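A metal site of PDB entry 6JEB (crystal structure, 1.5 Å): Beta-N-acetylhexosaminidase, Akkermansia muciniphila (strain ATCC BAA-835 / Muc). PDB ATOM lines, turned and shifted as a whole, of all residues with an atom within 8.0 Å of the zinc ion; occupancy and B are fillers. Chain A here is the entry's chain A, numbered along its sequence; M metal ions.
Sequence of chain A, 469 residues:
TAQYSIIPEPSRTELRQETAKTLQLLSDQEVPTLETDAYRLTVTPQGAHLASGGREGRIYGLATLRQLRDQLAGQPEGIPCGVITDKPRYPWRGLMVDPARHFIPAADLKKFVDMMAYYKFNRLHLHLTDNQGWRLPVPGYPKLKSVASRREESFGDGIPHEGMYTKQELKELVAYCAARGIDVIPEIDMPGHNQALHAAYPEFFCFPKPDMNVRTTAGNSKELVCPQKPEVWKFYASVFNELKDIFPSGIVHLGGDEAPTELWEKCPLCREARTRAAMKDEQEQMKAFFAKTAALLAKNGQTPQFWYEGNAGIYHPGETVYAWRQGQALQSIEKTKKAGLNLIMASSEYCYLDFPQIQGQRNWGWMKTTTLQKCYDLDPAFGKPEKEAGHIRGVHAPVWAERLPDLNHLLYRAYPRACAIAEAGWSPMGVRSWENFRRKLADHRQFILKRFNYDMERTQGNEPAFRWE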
ATOM      1  N   PHE A 204      19.316  15.832  29.678  1.00  0.00           N
ATOM      2  CA  PHE A 204      18.580  14.678  30.200  1.00  0.00           C
ATOM      3  C   PHE A 204      18.405  13.571  29.160  1.00  0.00           C
ATOM      4  O   PHE A 204      17.838  12.527  29.492  1.00  0.00           O
ATOM      5  CB  PHE A 204      17.174  15.074  30.674  1.00  0.00           C
ATOM      6  CG  PHE A 204      17.147  16.013  31.863  1.00  0.00           C
ATOM      7  CD1 PHE A 204      18.295  16.342  32.572  1.00  0.00           C
ATOM      8  CD2 PHE A 204      15.933  16.560  32.271  1.00  0.00           C
ATOM      9  CE1 PHE A 204      18.233  17.217  33.676  1.00  0.00           C
ATOM     10  CE2 PHE A 204      15.850  17.429  33.363  1.00  0.00           C
ATOM     11  CZ  PHE A 204      17.010  17.765  34.067  1.00  0.00           C
ATOM     12  N   PHE A 205      18.891  13.752  27.938  1.00  0.00           N
ATOM     13  CA  PHE A 205      18.550  12.896  26.813  1.00  0.00           C
ATOM     14  C   PHE A 205      19.785  12.186  26.275  1.00  0.00           C
ATOM     15  O   PHE A 205      20.914  12.655  26.431  1.00  0.00           O
ATOM     16  CB  PHE A 205      17.830  13.690  25.724  1.00  0.00           C
ATOM     17  CG  PHE A 205      16.491  14.198  26.176  1.00  0.00           C
ATOM     18  CD1 PHE A 205      16.391  15.302  27.023  1.00  0.00           C
ATOM     19  CD2 PHE A 205      15.335  13.518  25.813  1.00  0.00           C
ATOM     20  CE1 PHE A 205      15.149  15.730  27.488  1.00  0.00           C
ATOM     21  CE2 PHE A 205      14.089  13.945  26.269  1.00  0.00           C
ATOM     22  CZ  PHE A 205      13.995  15.056  27.102  1.00  0.00           C
ATOM     23  N   CYS A 206      19.548  11.044  25.608  1.00  0.00           N
ATOM     24  CA  CYS A 206      20.653  10.248  25.070  1.00  0.00           C
ATOM     25  C   CYS A 206      21.481  11.051  24.068  1.00  0.00           C
ATOM     26  O   CYS A 206      22.719  10.917  24.022  1.00  0.00           O
ATOM     27  CB  CYS A 206      20.106   8.991  24.385  1.00  0.00           C
ATOM     28  SG  CYS A 206      19.092   7.925  25.434  1.00  0.00           S
ATOM     29  N   PHE A 207      20.822  11.851  23.241  1.00  0.00           N
ATOM     30  CA  PHE A 207      21.464  12.631  22.180  1.00  0.00           C
ATOM     31  C   PHE A 207      21.087  14.091  22.379  1.00  0.00           C
ATOM     32  O   PHE A 207      20.160  14.600  21.734  1.00  0.00           O
ATOM     33  CB  PHE A 207      21.097  12.087  20.805  1.00  0.00           C
ATOM     34  CG  PHE A 207      21.591  10.688  20.555  1.00  0.00           C
ATOM     35  CD1 PHE A 207      22.881  10.469  20.093  1.00  0.00           C
ATOM     36  CD2 PHE A 207      20.788   9.584  20.830  1.00  0.00           C
ATOM     37  CE1 PHE A 207      23.361   9.187  19.888  1.00  0.00           C
ATOM     38  CE2 PHE A 207      21.266   8.293  20.627  1.00  0.00           C
ATOM     39  CZ  PHE A 207      22.555   8.102  20.143  1.00  0.00           C
ATOM     40  N   LEU A 224      13.789  10.337  23.963  1.00  0.00           N
ATOM     41  CA  LEU A 224      13.515   9.729  25.263  1.00  0.00           C
ATOM     42  C   LEU A 224      14.554  10.189  26.274  1.00  0.00           C
ATOM     43  O   LEU A 224      15.743  10.296  25.943  1.00  0.00           O
ATOM     44  CB  LEU A 224      13.570   8.196  25.167  1.00  0.00           C
ATOM     45  CG  LEU A 224      12.709   7.502  24.099  1.00  0.00           C
ATOM     46  CD1 LEU A 224      12.691   6.005  24.327  1.00  0.00           C
ATOM     47  CD2 LEU A 224      11.280   8.039  24.101  1.00  0.00           C
ATOM     48  N   VAL A 225      14.118  10.459  27.505  1.00  0.00           N
ATOM     49  CA  VAL A 225      15.090  10.704  28.568  1.00  0.00           C
ATOM     50  C   VAL A 225      16.002   9.480  28.689  1.00  0.00           C
ATOM     51  O   VAL A 225      15.596   8.336  28.443  1.00  0.00           O
ATOM     52  CB  VAL A 225      14.434  11.059  29.909  1.00  0.00           C
ATOM     53  CG1 VAL A 225      13.784  12.441  29.844  1.00  0.00           C
ATOM     54  CG2 VAL A 225      13.415   9.980  30.324  1.00  0.00           C
ATOM     55  N   CYS A 226      17.258   9.738  29.054  1.00  0.00           N
ATOM     56  CA  CYS A 226      18.237   8.668  29.143  1.00  0.00           C
ATOM     57  C   CYS A 226      18.262   8.121  30.568  1.00  0.00           C
ATOM     58  O   CYS A 226      18.657   8.846  31.490  1.00  0.00           O
ATOM     59  CB  CYS A 226      19.626   9.169  28.762  1.00  0.00           C
ATOM     60  SG  CYS A 226      20.863   7.847  28.841  1.00  0.00           S
ATOM     61  N   PRO A 227      17.869   6.860  30.800  1.00  0.00           N
ATOM     62  CA  PRO A 227      17.863   6.337  32.175  1.00  0.00           C
ATOM     63  C   PRO A 227      19.237   6.245  32.807  1.00  0.00           C
ATOM     64  O   PRO A 227      19.324   6.008  34.014  1.00  0.00           O
ATOM     65  CB  PRO A 227      17.241   4.936  32.026  1.00  0.00           C
ATOM     66  CG  PRO A 227      16.493   4.977  30.725  1.00  0.00           C
ATOM     67  CD  PRO A 227      17.308   5.895  29.836  1.00  0.00           C
ATOM     68  N   GLN A 228      20.320   6.396  32.034  1.00  0.00           N
ATOM     69  CA  GLN A 228      21.649   6.269  32.610  1.00  0.00           C
ATOM     70  C   GLN A 228      22.149   7.557  33.253  1.00  0.00           C
ATOM     71  O   GLN A 228      23.211   7.532  33.885  1.00  0.00           O
ATOM     72  CB  GLN A 228      22.657   5.841  31.543  1.00  0.00           C
ATOM     73  CG  GLN A 228      22.135   4.778  30.567  1.00  0.00           C
ATOM     74  CD  GLN A 228      21.298   3.697  31.225  1.00  0.00           C
ATOM     75  OE1 GLN A 228      21.544   3.295  32.376  1.00  0.00           O
ATOM     76  NE2 GLN A 228      20.303   3.212  30.509  1.00  0.00           N
ATOM     77  N   LYS A 229      21.419   8.647  33.121  1.00  0.00           N
ATOM     78  CA  LYS A 229      21.933   9.945  33.563  1.00  0.00           C
ATOM     79  C   LYS A 229      21.416  10.264  34.964  1.00  0.00           C
ATOM     80  O   LYS A 229      20.192  10.300  35.171  1.00  0.00           O
ATOM     81  CB  LYS A 229      21.517  11.027  32.580  1.00  0.00           C
ATOM     82  CG  LYS A 229      22.039  10.727  31.177  1.00  0.00           C
ATOM     83  CD  LYS A 229      22.343  11.995  30.425  1.00  0.00           C
ATOM     84  CE  LYS A 229      22.956  11.695  29.075  1.00  0.00           C
ATOM     85  NZ  LYS A 229      23.072  12.925  28.230  1.00  0.00           N
ATOM     86  N   LEU A 263      16.284   5.584  19.812  1.00  0.00           N
ATOM     87  CA  LEU A 263      17.413   6.331  20.362  1.00  0.00           C
ATOM     88  C   LEU A 263      18.025   5.633  21.580  1.00  0.00           C
ATOM     89  O   LEU A 263      19.237   5.745  21.794  1.00  0.00           O
ATOM     90  CB  LEU A 263      17.034   7.783  20.653  1.00  0.00           C
ATOM     91  CG  LEU A 263      16.671   8.613  19.419  1.00  0.00           C
ATOM     92  CD1 LEU A 263      16.524  10.097  19.779  1.00  0.00           C
ATOM     93  CD2 LEU A 263      17.690   8.430  18.308  1.00  0.00           C
ATOM     94  N   TRP A 264      17.205   4.938  22.388  1.00  0.00           N
ATOM     95  CA  TRP A 264      17.772   4.091  23.433  1.00  0.00           C
ATOM     96  C   TRP A 264      18.657   3.007  22.834  1.00  0.00           C
ATOM     97  O   TRP A 264      19.735   2.699  23.369  1.00  0.00           O
ATOM     98  CB  TRP A 264      16.665   3.437  24.260  1.00  0.00           C
ATOM     99  CG  TRP A 264      16.092   4.300  25.343  1.00  0.00           C
ATOM    100  CD1 TRP A 264      16.426   5.601  25.633  1.00  0.00           C
ATOM    101  CD2 TRP A 264      15.100   3.913  26.298  1.00  0.00           C
ATOM    102  NE1 TRP A 264      15.680   6.042  26.706  1.00  0.00           N
ATOM    103  CE2 TRP A 264      14.866   5.027  27.138  1.00  0.00           C
ATOM    104  CE3 TRP A 264      14.394   2.719  26.530  1.00  0.00           C
ATOM    105  CZ2 TRP A 264      13.953   4.988  28.185  1.00  0.00           C
ATOM    106  CZ3 TRP A 264      13.485   2.690  27.576  1.00  0.00           C
ATOM    107  CH2 TRP A 264      13.269   3.816  28.395  1.00  0.00           C
ATOM    108  N   GLU A 265      18.218   2.386  21.734  1.00  0.00           N
ATOM    109  CA  GLU A 265      19.034   1.351  21.106  1.00  0.00           C
ATOM    110  C   GLU A 265      20.388   1.892  20.699  1.00  0.00           C
ATOM    111  O   GLU A 265      21.408   1.212  20.868  1.00  0.00           O
ATOM    112  CB  GLU A 265      18.301   0.756  19.893  1.00  0.00           C
ATOM    113  CG  GLU A 265      18.938  -0.537  19.364  1.00  0.00           C
ATOM    114  CD  GLU A 265      20.183  -0.287  18.530  1.00  0.00           C
ATOM    115  OE1 GLU A 265      20.238   0.727  17.815  1.00  0.00           O
ATOM    116  OE2 GLU A 265      21.132  -1.116  18.609  1.00  0.00           O
ATOM    117  N   LYS A 266      20.419   3.119  20.161  1.00  0.00           N
ATOM    118  CA  LYS A 266      21.653   3.702  19.638  1.00  0.00           C
ATOM    119  C   LYS A 266      22.501   4.386  20.689  1.00  0.00           C
ATOM    120  O   LYS A 266      23.708   4.576  20.465  1.00  0.00           O
ATOM    121  CB  LYS A 266      21.317   4.746  18.565  1.00  0.00           C
ATOM    122  CG  LYS A 266      20.752   4.163  17.296  1.00  0.00           C
ATOM    123  CD  LYS A 266      20.385   5.239  16.298  1.00  0.00           C
ATOM    124  CE  LYS A 266      19.808   4.618  15.034  1.00  0.00           C
ATOM    125  NZ  LYS A 266      19.397   5.644  14.035  1.00  0.00           N
ATOM    126  N   CYS A 267      21.919   4.762  21.820  1.00  0.00           N
ATOM    127  CA  CYS A 267      22.625   5.549  22.826  1.00  0.00           C
ATOM    128  C   CYS A 267      23.857   4.808  23.335  1.00  0.00           C
ATOM    129  O   CYS A 267      23.757   3.651  23.764  1.00  0.00           O
ATOM    130  CB  CYS A 267      21.690   5.831  23.997  1.00  0.00           C
ATOM    131  SG  CYS A 267      22.502   6.621  25.412  1.00  0.00           S
ATOM    132  N   PRO A 268      25.043   5.437  23.327  1.00  0.00           N
ATOM    133  CA  PRO A 268      26.231   4.739  23.815  1.00  0.00           C
ATOM    134  C   PRO A 268      26.176   4.427  25.301  1.00  0.00           C
ATOM    135  O   PRO A 268      26.772   3.432  25.735  1.00  0.00           O
ATOM    136  CB  PRO A 268      27.386   5.700  23.470  1.00  0.00           C
ATOM    137  CG  PRO A 268      26.719   7.042  23.380  1.00  0.00           C
ATOM    138  CD  PRO A 268      25.359   6.778  22.810  1.00  0.00           C
ATOM    139  N   LEU A 269      25.470   5.238  26.091  1.00  0.00           N
ATOM    140  CA  LEU A 269      25.316   4.926  27.506  1.00  0.00           C
ATOM    141  C   LEU A 269      24.340   3.783  27.714  1.00  0.00           C
ATOM    142  O   LEU A 269      24.600   2.856  28.479  1.00  0.00           O
ATOM    143  CB  LEU A 269      24.838   6.160  28.276  1.00  0.00           C
ATOM    144  CG  LEU A 269      25.744   7.388  28.210  1.00  0.00           C
ATOM    145  CD1 LEU A 269      25.108   8.524  28.983  1.00  0.00           C
ATOM    146  CD2 LEU A 269      27.133   7.067  28.748  1.00  0.00           C
ATOM    147  N   CYS A 270      23.180   3.842  27.034  1.00  0.00           N
ATOM    148  CA  CYS A 270      22.182   2.795  27.200  1.00  0.00           C
ATOM    149  C   CYS A 270      22.665   1.446  26.674  1.00  0.00           C
ATOM    150  O   CYS A 270      22.320   0.409  27.251  1.00  0.00           O
ATOM    151  CB  CYS A 270      20.863   3.192  26.536  1.00  0.00           C
ATOM    152  SG  CYS A 270      19.992   4.560  27.375  1.00  0.00           S
ATOM    153  N   ARG A 271      23.461   1.444  25.598  1.00  0.00           N
ATOM    154  CA  ARG A 271      23.969   0.173  25.083  1.00  0.00           C
ATOM    155  C   ARG A 271      24.753  -0.581  26.150  1.00  0.00           C
ATOM    156  O   ARG A 271      24.540  -1.775  26.355  1.00  0.00           O
ATOM    157  CB  ARG A 271      24.851   0.418  23.854  1.00  0.00           C
ATOM    158  CG  ARG A 271      24.036   0.660  22.618  1.00  0.00           C
ATOM    159  CD  ARG A 271      24.917   1.031  21.450  1.00  0.00           C
ATOM    160  NE  ARG A 271      24.147   0.983  20.216  1.00  0.00           N
ATOM    161  CZ  ARG A 271      24.651   1.192  19.007  1.00  0.00           C
ATOM    162  NH1 ARG A 271      25.936   1.462  18.845  1.00  0.00           N
ATOM    163  NH2 ARG A 271      23.847   1.117  17.950  1.00  0.00           N
ATOM    164  N   ALA A 273      24.727   0.012  29.453  1.00  0.00           N
ATOM    165  CA  ALA A 273      23.874  -0.287  30.597  1.00  0.00           C
ATOM    166  C   ALA A 273      23.071  -1.559  30.357  1.00  0.00           C
ATOM    167  O   ALA A 273      22.914  -2.375  31.270  1.00  0.00           O
ATOM    168  CB  ALA A 273      22.946   0.883  30.881  1.00  0.00           C
ATOM    169  N   ARG A 274      22.573  -1.755  29.131  1.00  0.00           N
ATOM    170  CA  ARG A 274      21.878  -2.997  28.822  1.00  0.00           C
ATOM    171  C   ARG A 274      22.810  -4.199  28.921  1.00  0.00           C
ATOM    172  O   ARG A 274      22.412  -5.252  29.412  1.00  0.00           O
ATOM    173  CB  ARG A 274      21.233  -2.937  27.432  1.00  0.00           C
ATOM    174  CG  ARG A 274      20.010  -2.030  27.368  1.00  0.00           C
ATOM    175  CD  ARG A 274      19.238  -2.244  26.073  1.00  0.00           C
ATOM    176  NE  ARG A 274      20.068  -2.029  24.882  1.00  0.00           N
ATOM    177  CZ  ARG A 274      20.253  -0.847  24.305  1.00  0.00           C
ATOM    178  NH1 ARG A 274      19.686   0.252  24.813  1.00  0.00           N
ATOM    179  NH2 ARG A 274      21.033  -0.737  23.230  1.00  0.00           N
ATOM    180  N   GLN A 285      14.458  -2.729  28.861  1.00  0.00           N
ATOM    181  CA  GLN A 285      14.912  -1.444  29.380  1.00  0.00           C
ATOM    182  C   GLN A 285      13.741  -0.588  29.820  1.00  0.00           C
ATOM    183  O   GLN A 285      13.793   0.073  30.868  1.00  0.00           O
ATOM    184  CB  GLN A 285      15.750  -0.726  28.325  1.00  0.00           C
ATOM    185  CG  GLN A 285      16.436   0.502  28.889  1.00  0.00           C
ATOM    186  CD  GLN A 285      17.300   1.216  27.864  1.00  0.00           C
ATOM    187  OE1 GLN A 285      17.716   0.636  26.862  1.00  0.00           O
ATOM    188  NE2 GLN A 285      17.574   2.490  28.129  1.00  0.00           N
HETATM  189 ZN    ZN M   1      20.620   6.765  26.782  1.00  0.00          ZN
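Along chain A the residues within 4 Å of the zinc ion span positions 206 to 270. The nearest printed residue that does not touch the zinc ion is Trp 264 (4.5 Å).
The zinc ion is bound by the side-chain sulfur (SG) of Cys 267 (2.3 Å), the side-chain sulfur (SG) of Cys 226 (2.3 Å), the side-chain sulfur (SG) of Cys 206 (2.3 Å) and the side-chain sulfur (SG) of Cys 270 (2.4 Å). The zinc ion has four donor atoms within binding distance.
SG of Cys 267 sits close to N of Leu 269. The side-chain sulfur (SG) of Cys 226 lies close to the backbone NH (N) of Gln 228 (3.5 Å). The backbone NH (N) of Cys 226 is in hydrogen-bond range of the backbone carbonyl oxygen (O) of Phe 204 (2.9 Å). The side-chain sulfur of Cys 270 lies close to the side-chain amide nitrogen of Gln 228, at 3.4 Å. The side-chain sulfur (SG) of Cys 270 sits close to the side-chain amide nitrogen (NE2) of Gln 285, 3.3 Å away.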
